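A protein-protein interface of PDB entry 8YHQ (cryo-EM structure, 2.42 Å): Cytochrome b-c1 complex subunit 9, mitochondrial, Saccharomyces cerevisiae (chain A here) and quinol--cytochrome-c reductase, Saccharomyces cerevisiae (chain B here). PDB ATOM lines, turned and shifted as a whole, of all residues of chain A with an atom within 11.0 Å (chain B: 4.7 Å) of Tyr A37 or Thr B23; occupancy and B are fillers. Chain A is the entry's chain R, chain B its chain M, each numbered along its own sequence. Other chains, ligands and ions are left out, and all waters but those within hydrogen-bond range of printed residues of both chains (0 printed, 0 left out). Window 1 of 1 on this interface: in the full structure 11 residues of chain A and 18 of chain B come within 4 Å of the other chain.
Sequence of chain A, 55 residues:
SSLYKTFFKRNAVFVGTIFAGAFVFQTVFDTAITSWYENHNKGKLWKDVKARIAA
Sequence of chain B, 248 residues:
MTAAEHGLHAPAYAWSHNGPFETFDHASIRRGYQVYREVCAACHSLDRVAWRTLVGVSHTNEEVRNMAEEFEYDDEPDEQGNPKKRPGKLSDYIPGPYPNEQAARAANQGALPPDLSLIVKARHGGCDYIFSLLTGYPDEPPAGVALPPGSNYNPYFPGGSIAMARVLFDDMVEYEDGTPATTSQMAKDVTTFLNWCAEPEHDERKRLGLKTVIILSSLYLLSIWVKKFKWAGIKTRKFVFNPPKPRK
Of the 11 printed residues of chain B, 8 touch a printed residue of chain A. Printed residues of chain A that touch a printed residue of chain B: Thr A34, Tyr A37, His A40, Asn A41 and Lys A44. Among the printed residues, Asp or Glu carboxylates within 4 Å of a Lys or Arg side-chain nitrogen of the other chain: Lys A44 with Glu B22.
OG1 of Thr A34 lies within hydrogen-bond range of O of Asp A30 (2.7 Å). A ring nitrogen (ND1) of His B202 sits at hydrogen-bond distance from the side-chain carboxylate (OD1) of Asp B203, 2.8 Å away. The backbone carbonyl oxygen of Tyr A37 is in hydrogen-bond range of the side-chain amide nitrogen of Asn A41, 3.5 Å away. The backbone NH (N) of Phe B24 sits at hydrogen-bond distance from the side-chain carboxylate (OD1) of Asp B203 (3.3 Å). The side-chain amino group of Lys B206 lies within hydrogen-bond range of a ring nitrogen (NE2) of His B202, at 3.2 Å. The side-chain amino group (NZ) of Lys B206 sits at hydrogen-bond distance from the backbone carbonyl oxygen (O) of His B17 (2.9 Å).
Of the printed residues of chain B, His A40 touches Phe B21 (3.6 Å) and Glu B22 (3.5 Å). Of the printed residues of chain B, Lys A44 touches Ser B16, Glu B22, Thr B23 and Phe B24. Of chain A, only Lys A44 comes within 4 Å of Ser B16. His B17 touches none of the printed residues of chain A. Glu B22 touches just these residues of chain A: Tyr A37, His A40, Asn A41 and Lys A44. Of chain A, only Tyr A37, Asn A41 and Lys A44 come within 4 Å of Thr B23. Phe B24 touches just one residue of chain A: Lys A44. Of chain A, only Tyr A37 comes within 4 Å of Asp B203. The nearest printed residue of chain B that does not touch Tyr A37 is His B202 (5.0 Å). The nearest residue of chain A that does not touch Thr B23 is Leu A45 (4.5 Å).
Among the printed residues, pairs that only touch across the chains: Tyr A37 with Lys B206 (3.4 Å), Tyr A37 with Phe B21 (3.5 Å), Lys A44 with Thr B23 (3.5 Å), His A40 with Glu B22 (3.5 Å), Lys A44 with Phe B24 (3.5 Å), Tyr A37 with Asp B203 (3.6 Å), His A40 with Phe B21 (3.6 Å), Tyr A37 with Thr B23 (3.6 Å), Tyr A37 with Arg B207 (3.7 Å) and Thr A34 with Arg B207 (3.8 Å).
N of Thr B23 is in hydrogen-bond range of OD1 of Asn A41. The side-chain hydroxyl (OH) of Tyr A37 lies within hydrogen-bond range of the backbone carbonyl oxygen (O) of Glu B22. OE1 of Glu B22 sits close to OD1 of Asn A41. OE1 of Glu B22 lies within salt-bridge range of NZ of Lys A44 (3.1 Å). ND2 of Asn A41 lies within hydrogen-bond range of O of Phe B21, 2.7 Å away. The backbone carbonyl oxygen (O) of Ser B16 is in hydrogen-bond range of the side-chain amino group (NZ) of Lys A44, 3.0 Å away.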
ATOM      1  N   PHE A  29      30.696   2.613 -18.275  1.00  0.00           N
ATOM      2  CA  PHE A  29      29.390   2.146 -17.827  1.00  0.00           C
ATOM      3  C   PHE A  29      28.286   3.082 -18.298  1.00  0.00           C
ATOM      4  O   PHE A  29      27.204   2.631 -18.689  1.00  0.00           O
ATOM      5  CB  PHE A  29      29.398   2.012 -16.306  1.00  0.00           C
ATOM      6  CG  PHE A  29      28.129   1.489 -15.729  1.00  0.00           C
ATOM      7  CD1 PHE A  29      27.713   0.203 -15.988  1.00  0.00           C
ATOM      8  CD2 PHE A  29      27.364   2.278 -14.898  1.00  0.00           C
ATOM      9  CE1 PHE A  29      26.549  -0.279 -15.446  1.00  0.00           C
ATOM     10  CE2 PHE A  29      26.203   1.800 -14.360  1.00  0.00           C
ATOM     11  CZ  PHE A  29      25.794   0.521 -14.629  1.00  0.00           C
ATOM     12  N   ASP A  30      28.543   4.391 -18.277  1.00  0.00           N
ATOM     13  CA  ASP A  30      27.571   5.356 -18.776  1.00  0.00           C
ATOM     14  C   ASP A  30      27.310   5.161 -20.264  1.00  0.00           C
ATOM     15  O   ASP A  30      26.156   5.068 -20.697  1.00  0.00           O
ATOM     16  CB  ASP A  30      28.070   6.775 -18.505  1.00  0.00           C
ATOM     17  CG  ASP A  30      27.078   7.835 -18.933  1.00  0.00           C
ATOM     18  OD1 ASP A  30      25.989   7.912 -18.331  1.00  0.00           O
ATOM     19  OD2 ASP A  30      27.391   8.599 -19.869  1.00  0.00           O
ATOM     20  N   THR A  31      28.378   5.115 -21.065  1.00  0.00           N
ATOM     21  CA  THR A  31      28.241   4.986 -22.512  1.00  0.00           C
ATOM     22  C   THR A  31      27.509   3.706 -22.900  1.00  0.00           C
ATOM     23  O   THR A  31      26.764   3.686 -23.886  1.00  0.00           O
ATOM     24  CB  THR A  31      29.625   5.035 -23.162  1.00  0.00           C
ATOM     25  OG1 THR A  31      30.214   6.321 -22.944  1.00  0.00           O
ATOM     26  CG2 THR A  31      29.544   4.773 -24.649  1.00  0.00           C
ATOM     27  N   ALA A  32      27.705   2.630 -22.138  1.00  0.00           N
ATOM     28  CA  ALA A  32      27.097   1.352 -22.488  1.00  0.00           C
ATOM     29  C   ALA A  32      25.599   1.346 -22.215  1.00  0.00           C
ATOM     30  O   ALA A  32      24.816   0.836 -23.023  1.00  0.00           O
ATOM     31  CB  ALA A  32      27.779   0.226 -21.720  1.00  0.00           C
ATOM     32  N   ILE A  33      25.181   1.895 -21.076  1.00  0.00           N
ATOM     33  CA  ILE A  33      23.767   1.876 -20.718  1.00  0.00           C
ATOM     34  C   ILE A  33      22.981   2.820 -21.616  1.00  0.00           C
ATOM     35  O   ILE A  33      21.860   2.512 -22.039  1.00  0.00           O
ATOM     36  CB  ILE A  33      23.577   2.236 -19.232  1.00  0.00           C
ATOM     37  CG1 ILE A  33      24.324   1.267 -18.310  1.00  0.00           C
ATOM     38  CG2 ILE A  33      22.099   2.271 -18.883  1.00  0.00           C
ATOM     39  CD1 ILE A  33      23.693  -0.091 -18.164  1.00  0.00           C
ATOM     40  N   THR A  34      23.489   4.003 -21.954  1.00  0.00           N
ATOM     41  CA  THR A  34      22.864   5.004 -22.831  1.00  0.00           C
ATOM     42  C   THR A  34      22.783   4.498 -24.254  1.00  0.00           C
ATOM     43  O   THR A  34      21.921   4.958 -24.952  1.00  0.00           O
ATOM     44  CB  THR A  34      23.590   6.361 -22.905  1.00  0.00           C
ATOM     45  OG1 THR A  34      24.225   6.659 -21.674  1.00  0.00           O
ATOM     46  CG2 THR A  34      22.676   7.503 -23.265  1.00  0.00           C
ATOM     47  N   SER A  35      23.627   3.600 -24.680  1.00  0.00           N
ATOM     48  CA  SER A  35      23.476   3.011 -26.004  1.00  0.00           C
ATOM     49  C   SER A  35      22.398   1.934 -26.020  1.00  0.00           C
ATOM     50  O   SER A  35      21.670   1.792 -27.008  1.00  0.00           O
ATOM     51  CB  SER A  35      24.813   2.445 -26.476  1.00  0.00           C
ATOM     52  OG  SER A  35      24.687   1.828 -27.739  1.00  0.00           O
ATOM     53  N   TRP A  36      22.281   1.161 -24.940  1.00  0.00           N
ATOM     54  CA  TRP A  36      21.259   0.122 -24.884  1.00  0.00           C
ATOM     55  C   TRP A  36      19.865   0.722 -24.777  1.00  0.00           C
ATOM     56  O   TRP A  36      18.912   0.203 -25.367  1.00  0.00           O
ATOM     57  CB  TRP A  36      21.530  -0.817 -23.710  1.00  0.00           C
ATOM     58  CG  TRP A  36      20.592  -1.969 -23.634  1.00  0.00           C
ATOM     59  CD1 TRP A  36      20.767  -3.197 -24.187  1.00  0.00           C
ATOM     60  CD2 TRP A  36      19.326  -2.006 -22.970  1.00  0.00           C
ATOM     61  NE1 TRP A  36      19.691  -3.997 -23.914  1.00  0.00           N
ATOM     62  CE2 TRP A  36      18.791  -3.288 -23.167  1.00  0.00           C
ATOM     63  CE3 TRP A  36      18.591  -1.078 -22.229  1.00  0.00           C
ATOM     64  CZ2 TRP A  36      17.562  -3.666 -22.652  1.00  0.00           C
ATOM     65  CZ3 TRP A  36      17.378  -1.454 -21.723  1.00  0.00           C
ATOM     66  CH2 TRP A  36      16.871  -2.735 -21.933  1.00  0.00           C
ATOM     67  N   TYR A  37      19.727   1.811 -24.019  1.00  0.00           N
ATOM     68  CA  TYR A  37      18.426   2.441 -23.830  1.00  0.00           C
ATOM     69  C   TYR A  37      17.943   3.097 -25.117  1.00  0.00           C
ATOM     70  O   TYR A  37      16.794   2.911 -25.529  1.00  0.00           O
ATOM     71  CB  TYR A  37      18.524   3.463 -22.697  1.00  0.00           C
ATOM     72  CG  TYR A  37      17.210   3.939 -22.130  1.00  0.00           C
ATOM     73  CD1 TYR A  37      16.389   3.086 -21.415  1.00  0.00           C
ATOM     74  CD2 TYR A  37      16.807   5.255 -22.284  1.00  0.00           C
ATOM     75  CE1 TYR A  37      15.200   3.526 -20.886  1.00  0.00           C
ATOM     76  CE2 TYR A  37      15.619   5.700 -21.760  1.00  0.00           C
ATOM     77  CZ  TYR A  37      14.821   4.832 -21.062  1.00  0.00           C
ATOM     78  OH  TYR A  37      13.635   5.269 -20.534  1.00  0.00           O
ATOM     79  N   GLU A  38      18.815   3.869 -25.768  1.00  0.00           N
ATOM     80  CA  GLU A  38      18.452   4.548 -27.003  1.00  0.00           C
ATOM     81  C   GLU A  38      18.155   3.584 -28.146  1.00  0.00           C
ATOM     82  O   GLU A  38      17.429   3.956 -29.071  1.00  0.00           O
ATOM     83  CB  GLU A  38      19.566   5.506 -27.414  1.00  0.00           C
ATOM     84  CG  GLU A  38      19.608   6.792 -26.617  1.00  0.00           C
ATOM     85  CD  GLU A  38      20.815   7.651 -26.940  1.00  0.00           C
ATOM     86  OE1 GLU A  38      21.702   7.184 -27.685  1.00  0.00           O
ATOM     87  OE2 GLU A  38      20.878   8.796 -26.447  1.00  0.00           O
ATOM     88  N   ASN A  39      18.695   2.367 -28.107  1.00  0.00           N
ATOM     89  CA  ASN A  39      18.416   1.368 -29.133  1.00  0.00           C
ATOM     90  C   ASN A  39      17.153   0.570 -28.851  1.00  0.00           C
ATOM     91  O   ASN A  39      16.459   0.170 -29.792  1.00  0.00           O
ATOM     92  CB  ASN A  39      19.604   0.411 -29.274  1.00  0.00           C
ATOM     93  CG  ASN A  39      19.276  -0.805 -30.111  1.00  0.00           C
ATOM     94  OD1 ASN A  39      19.022  -0.695 -31.309  1.00  0.00           O
ATOM     95  ND2 ASN A  39      19.270  -1.971 -29.484  1.00  0.00           N
ATOM     96  N   HIS A  40      16.837   0.329 -27.580  1.00  0.00           N
ATOM     97  CA  HIS A  40      15.619  -0.391 -27.232  1.00  0.00           C
ATOM     98  C   HIS A  40      14.370   0.411 -27.579  1.00  0.00           C
ATOM     99  O   HIS A  40      13.309  -0.173 -27.824  1.00  0.00           O
ATOM    100  CB  HIS A  40      15.647  -0.736 -25.742  1.00  0.00           C
ATOM    101  CG  HIS A  40      14.434  -1.460 -25.253  1.00  0.00           C
ATOM    102  ND1 HIS A  40      14.323  -2.832 -25.279  1.00  0.00           N
ATOM    103  CD2 HIS A  40      13.289  -1.001 -24.698  1.00  0.00           C
ATOM    104  CE1 HIS A  40      13.155  -3.187 -24.772  1.00  0.00           C
ATOM    105  NE2 HIS A  40      12.510  -2.094 -24.412  1.00  0.00           N
ATOM    106  N   ASN A  41      14.479   1.738 -27.611  1.00  0.00           N
ATOM    107  CA  ASN A  41      13.366   2.645 -27.871  1.00  0.00           C
ATOM    108  C   ASN A  41      13.515   3.334 -29.228  1.00  0.00           C
ATOM    109  O   ASN A  41      13.236   4.524 -29.378  1.00  0.00           O
ATOM    110  CB  ASN A  41      13.255   3.667 -26.742  1.00  0.00           C
ATOM    111  CG  ASN A  41      12.668   3.076 -25.480  1.00  0.00           C
ATOM    112  OD1 ASN A  41      11.499   2.703 -25.441  1.00  0.00           O
ATOM    113  ND2 ASN A  41      13.481   2.984 -24.439  1.00  0.00           N
ATOM    114  N   LYS A  42      13.954   2.584 -30.234  1.00  0.00           N
ATOM    115  CA  LYS A  42      14.184   3.136 -31.562  1.00  0.00           C
ATOM    116  C   LYS A  42      12.861   3.340 -32.289  1.00  0.00           C
ATOM    117  O   LYS A  42      12.024   2.434 -32.340  1.00  0.00           O
ATOM    118  CB  LYS A  42      15.089   2.210 -32.367  1.00  0.00           C
ATOM    119  CG  LYS A  42      15.759   2.864 -33.551  1.00  0.00           C
ATOM    120  CD  LYS A  42      16.683   1.886 -34.265  1.00  0.00           C
ATOM    121  CE  LYS A  42      17.756   2.583 -35.098  1.00  0.00           C
ATOM    122  NZ  LYS A  42      17.294   2.875 -36.482  1.00  0.00           N
ATOM    123  N   GLY A  43      12.679   4.535 -32.854  1.00  0.00           N
ATOM    124  CA  GLY A  43      11.462   4.915 -33.532  1.00  0.00           C
ATOM    125  C   GLY A  43      10.559   5.833 -32.736  1.00  0.00           C
ATOM    126  O   GLY A  43       9.639   6.421 -33.312  1.00  0.00           O
ATOM    127  N   LYS A  44      10.794   5.962 -31.430  1.00  0.00           N
ATOM    128  CA  LYS A  44      10.057   6.883 -30.577  1.00  0.00           C
ATOM    129  C   LYS A  44      10.789   8.188 -30.329  1.00  0.00           C
ATOM    130  O   LYS A  44      10.144   9.195 -30.034  1.00  0.00           O
ATOM    131  CB  LYS A  44       9.784   6.251 -29.215  1.00  0.00           C
ATOM    132  CG  LYS A  44       8.898   5.047 -29.202  1.00  0.00           C
ATOM    133  CD  LYS A  44       8.875   4.484 -27.801  1.00  0.00           C
ATOM    134  CE  LYS A  44       8.096   3.226 -27.699  1.00  0.00           C
ATOM    135  NZ  LYS A  44       8.093   2.755 -26.295  1.00  0.00           N
ATOM    136  N   LEU A  45      12.113   8.190 -30.422  1.00  0.00           N
ATOM    137  CA  LEU A  45      12.894   9.334 -29.990  1.00  0.00           C
ATOM    138  C   LEU A  45      12.658  10.525 -30.910  1.00  0.00           C
ATOM    139  O   LEU A  45      12.137  10.399 -32.020  1.00  0.00           O
ATOM    140  CB  LEU A  45      14.381   8.986 -29.957  1.00  0.00           C
ATOM    141  CG  LEU A  45      14.816   7.760 -29.153  1.00  0.00           C
ATOM    142  CD1 LEU A  45      16.260   7.440 -29.438  1.00  0.00           C
ATOM    143  CD2 LEU A  45      14.624   7.968 -27.673  1.00  0.00           C
ATOM    144  N   TRP A  46      13.049  11.702 -30.424  1.00  0.00           N
ATOM    145  CA  TRP A  46      12.851  12.919 -31.200  1.00  0.00           C
ATOM    146  C   TRP A  46      13.832  13.007 -32.360  1.00  0.00           C
ATOM    147  O   TRP A  46      13.477  13.490 -33.442  1.00  0.00           O
ATOM    148  CB  TRP A  46      12.985  14.146 -30.303  1.00  0.00           C
ATOM    149  CG  TRP A  46      13.169  15.412 -31.066  1.00  0.00           C
ATOM    150  CD1 TRP A  46      14.270  16.209 -31.073  1.00  0.00           C
ATOM    151  CD2 TRP A  46      12.225  16.028 -31.948  1.00  0.00           C
ATOM    152  NE1 TRP A  46      14.074  17.280 -31.901  1.00  0.00           N
ATOM    153  CE2 TRP A  46      12.825  17.193 -32.452  1.00  0.00           C
ATOM    154  CE3 TRP A  46      10.932  15.704 -32.365  1.00  0.00           C
ATOM    155  CZ2 TRP A  46      12.178  18.036 -33.345  1.00  0.00           C
ATOM    156  CZ3 TRP A  46      10.296  16.539 -33.250  1.00  0.00           C
ATOM    157  CH2 TRP A  46      10.917  17.691 -33.731  1.00  0.00           C
ATOM    158  N   LYS A  47      15.067  12.546 -32.164  1.00  0.00           N
ATOM    159  CA  LYS A  47      16.074  12.651 -33.210  1.00  0.00           C
ATOM    160  C   LYS A  47      15.756  11.784 -34.419  1.00  0.00           C
ATOM    161  O   LYS A  47      16.315  12.027 -35.493  1.00  0.00           O
ATOM    162  CB  LYS A  47      17.452  12.296 -32.649  1.00  0.00           C
ATOM    163  CG  LYS A  47      17.718  10.813 -32.455  1.00  0.00           C
ATOM    164  CD  LYS A  47      18.973  10.578 -31.621  1.00  0.00           C
ATOM    165  CE  LYS A  47      19.032   9.160 -31.077  1.00  0.00           C
ATOM    166  NZ  LYS A  47      20.418   8.707 -30.796  1.00  0.00           N
ATOM    167  N   ASP A  48      14.876  10.795 -34.275  1.00  0.00           N
ATOM    168  CA  ASP A  48      14.414   9.966 -35.378  1.00  0.00           C
ATOM    169  C   ASP A  48      13.123  10.479 -35.995  1.00  0.00           C
ATOM    170  O   ASP A  48      12.986  10.478 -37.221  1.00  0.00           O
ATOM    171  CB  ASP A  48      14.209   8.526 -34.902  1.00  0.00           C
ATOM    172  CG  ASP A  48      15.420   7.971 -34.182  1.00  0.00           C
ATOM    173  OD1 ASP A  48      16.509   7.929 -34.790  1.00  0.00           O
ATOM    174  OD2 ASP A  48      15.283   7.576 -33.006  1.00  0.00           O
ATOM    175  N   VAL A  49      12.167  10.900 -35.166  1.00  0.00           N
ATOM    176  CA  VAL A  49      10.968  11.561 -35.668  1.00  0.00           C
ATOM    177  C   VAL A  49      11.349  12.787 -36.484  1.00  0.00           C
ATOM    178  O   VAL A  49      10.801  13.025 -37.566  1.00  0.00           O
ATOM    179  CB  VAL A  49      10.033  11.920 -34.495  1.00  0.00           C
ATOM    180  CG1 VAL A  49       8.969  12.913 -34.918  1.00  0.00           C
ATOM    181  CG2 VAL A  49       9.386  10.671 -33.939  1.00  0.00           C
ATOM    182  N   ARG A  52      12.097  11.828 -39.925  1.00  0.00           N
ATOM    183  CA  ARG A  52      10.951  11.381 -40.705  1.00  0.00           C
ATOM    184  C   ARG A  52      10.080  12.547 -41.148  1.00  0.00           C
ATOM    185  O   ARG A  52       9.463  12.474 -42.217  1.00  0.00           O
ATOM    186  CB  ARG A  52      10.138  10.366 -39.903  1.00  0.00           C
ATOM    187  CG  ARG A  52      10.740   8.963 -39.927  1.00  0.00           C
ATOM    188  CD  ARG A  52      10.236   8.079 -38.803  1.00  0.00           C
ATOM    189  NE  ARG A  52       8.900   8.461 -38.343  1.00  0.00           N
ATOM    190  CZ  ARG A  52       8.428   8.271 -37.113  1.00  0.00           C
ATOM    191  NH1 ARG A  52       9.156   7.685 -36.168  1.00  0.00           N
ATOM    192  NH2 ARG A  52       7.196   8.667 -36.826  1.00  0.00           N
ATOM    193  N   SER B  16       2.136   2.800 -24.713  1.00  0.00           N
ATOM    194  CA  SER B  16       3.476   2.522 -25.205  1.00  0.00           C
ATOM    195  C   SER B  16       4.588   3.005 -24.281  1.00  0.00           C
ATOM    196  O   SER B  16       5.741   2.616 -24.486  1.00  0.00           O
ATOM    197  CB  SER B  16       3.653   3.162 -26.577  1.00  0.00           C
ATOM    198  OG  SER B  16       4.972   3.015 -27.045  1.00  0.00           O
ATOM    199  N   HIS B  17       4.277   3.830 -23.283  1.00  0.00           N
ATOM    200  CA  HIS B  17       5.263   4.323 -22.327  1.00  0.00           C
ATOM    201  C   HIS B  17       5.185   3.611 -20.983  1.00  0.00           C
ATOM    202  O   HIS B  17       5.964   3.933 -20.082  1.00  0.00           O
ATOM    203  CB  HIS B  17       5.120   5.838 -22.121  1.00  0.00           C
ATOM    204  CG  HIS B  17       3.720   6.293 -21.853  1.00  0.00           C
ATOM    205  ND1 HIS B  17       3.078   6.068 -20.656  1.00  0.00           N
ATOM    206  CD2 HIS B  17       2.835   6.954 -22.634  1.00  0.00           C
ATOM    207  CE1 HIS B  17       1.860   6.568 -20.713  1.00  0.00           C
ATOM    208  NE2 HIS B  17       1.687   7.114 -21.900  1.00  0.00           N
ATOM    209  N   PHE B  21      11.545   0.228 -19.146  1.00  0.00           N
ATOM    210  CA  PHE B  21      12.549   0.555 -20.153  1.00  0.00           C
ATOM    211  C   PHE B  21      11.989   1.369 -21.318  1.00  0.00           C
ATOM    212  O   PHE B  21      12.705   1.591 -22.299  1.00  0.00           O
ATOM    213  CB  PHE B  21      13.194  -0.725 -20.687  1.00  0.00           C
ATOM    214  CG  PHE B  21      13.605  -1.689 -19.622  1.00  0.00           C
ATOM    215  CD1 PHE B  21      14.454  -1.302 -18.607  1.00  0.00           C
ATOM    216  CD2 PHE B  21      13.146  -2.991 -19.637  1.00  0.00           C
ATOM    217  CE1 PHE B  21      14.823  -2.189 -17.631  1.00  0.00           C
ATOM    218  CE2 PHE B  21      13.516  -3.876 -18.664  1.00  0.00           C
ATOM    219  CZ  PHE B  21      14.356  -3.474 -17.660  1.00  0.00           C
ATOM    220  N   GLU B  22      10.744   1.830 -21.231  1.00  0.00           N
ATOM    221  CA  GLU B  22      10.074   2.521 -22.322  1.00  0.00           C
ATOM    222  C   GLU B  22      10.179   4.036 -22.184  1.00  0.00           C
ATOM    223  O   GLU B  22      10.360   4.572 -21.089  1.00  0.00           O
ATOM    224  CB  GLU B  22       8.603   2.128 -22.380  1.00  0.00           C
ATOM    225  CG  GLU B  22       8.326   0.646 -22.370  1.00  0.00           C
ATOM    226  CD  GLU B  22       9.005  -0.095 -23.496  1.00  0.00           C
ATOM    227  OE1 GLU B  22       9.293   0.530 -24.536  1.00  0.00           O
ATOM    228  OE2 GLU B  22       9.250  -1.309 -23.345  1.00  0.00           O
ATOM    229  N   THR B  23      10.056   4.719 -23.320  1.00  0.00           N
ATOM    230  CA  THR B  23      10.032   6.171 -23.418  1.00  0.00           C
ATOM    231  C   THR B  23       8.689   6.629 -23.970  1.00  0.00           C
ATOM    232  O   THR B  23       7.857   5.826 -24.395  1.00  0.00           O
ATOM    233  CB  THR B  23      11.154   6.693 -24.321  1.00  0.00           C
ATOM    234  OG1 THR B  23      11.044   6.104 -25.620  1.00  0.00           O
ATOM    235  CG2 THR B  23      12.492   6.391 -23.742  1.00  0.00           C
ATOM    236  N   PHE B  24       8.481   7.945 -23.955  1.00  0.00           N
ATOM    237  CA  PHE B  24       7.351   8.536 -24.658  1.00  0.00           C
ATOM    238  C   PHE B  24       7.524   8.387 -26.163  1.00  0.00           C
ATOM    239  O   PHE B  24       8.638   8.444 -26.687  1.00  0.00           O
ATOM    240  CB  PHE B  24       7.217  10.026 -24.328  1.00  0.00           C
ATOM    241  CG  PHE B  24       6.620  10.335 -22.979  1.00  0.00           C
ATOM    242  CD1 PHE B  24       5.481   9.706 -22.521  1.00  0.00           C
ATOM    243  CD2 PHE B  24       7.192  11.304 -22.181  1.00  0.00           C
ATOM    244  CE1 PHE B  24       4.958  10.014 -21.290  1.00  0.00           C
ATOM    245  CE2 PHE B  24       6.664  11.608 -20.964  1.00  0.00           C
ATOM    246  CZ  PHE B  24       5.553  10.965 -20.520  1.00  0.00           C
ATOM    247  N   ASP B  25       6.406   8.198 -26.858  1.00  0.00           N
ATOM    248  CA  ASP B  25       6.361   8.287 -28.314  1.00  0.00           C
ATOM    249  C   ASP B  25       6.229   9.751 -28.711  1.00  0.00           C
ATOM    250  O   ASP B  25       5.182  10.368 -28.497  1.00  0.00           O
ATOM    251  CB  ASP B  25       5.203   7.454 -28.850  1.00  0.00           C
ATOM    252  CG  ASP B  25       5.167   7.395 -30.365  1.00  0.00           C
ATOM    253  OD1 ASP B  25       6.107   7.891 -31.017  1.00  0.00           O
ATOM    254  OD2 ASP B  25       4.188   6.845 -30.907  1.00  0.00           O
ATOM    255  N   HIS B 202      10.364  12.100 -17.473  1.00  0.00           N
ATOM    256  CA  HIS B 202      10.035  10.684 -17.537  1.00  0.00           C
ATOM    257  C   HIS B 202      11.127   9.859 -18.213  1.00  0.00           C
ATOM    258  O   HIS B 202      11.474   8.771 -17.744  1.00  0.00           O
ATOM    259  CB  HIS B 202       8.701  10.569 -18.264  1.00  0.00           C
ATOM    260  CG  HIS B 202       8.299   9.183 -18.627  1.00  0.00           C
ATOM    261  ND1 HIS B 202       8.709   8.570 -19.788  1.00  0.00           N
ATOM    262  CD2 HIS B 202       7.461   8.316 -18.018  1.00  0.00           C
ATOM    263  CE1 HIS B 202       8.167   7.369 -19.861  1.00  0.00           C
ATOM    264  NE2 HIS B 202       7.406   7.191 -18.799  1.00  0.00           N
ATOM    265  N   ASP B 203      11.689  10.363 -19.312  1.00  0.00           N
ATOM    266  CA  ASP B 203      12.633   9.572 -20.090  1.00  0.00           C
ATOM    267  C   ASP B 203      14.017   9.538 -19.452  1.00  0.00           C
ATOM    268  O   ASP B 203      14.680   8.497 -19.472  1.00  0.00           O
ATOM    269  CB  ASP B 203      12.720  10.115 -21.516  1.00  0.00           C
ATOM    270  CG  ASP B 203      11.436   9.919 -22.302  1.00  0.00           C
ATOM    271  OD1 ASP B 203      10.482   9.325 -21.763  1.00  0.00           O
ATOM    272  OD2 ASP B 203      11.379  10.359 -23.466  1.00  0.00           O
ATOM    273  N   LYS B 206      13.989   7.200 -16.098  1.00  0.00           N
ATOM    274  CA  LYS B 206      13.930   5.755 -16.250  1.00  0.00           C
ATOM    275  C   LYS B 206      15.253   5.129 -16.675  1.00  0.00           C
ATOM    276  O   LYS B 206      15.390   3.908 -16.557  1.00  0.00           O
ATOM    277  CB  LYS B 206      12.844   5.391 -17.252  1.00  0.00           C
ATOM    278  CG  LYS B 206      11.445   5.363 -16.670  1.00  0.00           C
ATOM    279  CD  LYS B 206      10.423   5.135 -17.746  1.00  0.00           C
ATOM    280  CE  LYS B 206       9.192   4.470 -17.228  1.00  0.00           C
ATOM    281  NZ  LYS B 206       8.258   4.112 -18.307  1.00  0.00           N
ATOM    282  N   ARG B 207      16.171   5.945 -17.111  1.00  0.00           N
ATOM    283  CA  ARG B 207      17.482   5.564 -17.628  1.00  0.00           C
ATOM    284  C   ARG B 207      18.530   5.705 -16.516  1.00  0.00           C
ATOM    285  O   ARG B 207      19.440   4.934 -16.553  1.00  0.00           O
ATOM    286  CB  ARG B 207      17.793   6.421 -18.867  1.00  0.00           C
ATOM    287  CG  ARG B 207      19.126   6.101 -19.513  1.00  0.00           C
ATOM    288  CD  ARG B 207      19.585   7.208 -20.413  1.00  0.00           C
ATOM    289  NE  ARG B 207      20.829   7.778 -19.965  1.00  0.00           N
ATOM    290  CZ  ARG B 207      20.952   8.925 -19.333  1.00  0.00           C
ATOM    291  NH1 ARG B 207      21.974   9.129 -18.531  1.00  0.00           N
ATOM    292  NH2 ARG B 207      20.056   9.870 -19.512  1.00  0.00           N
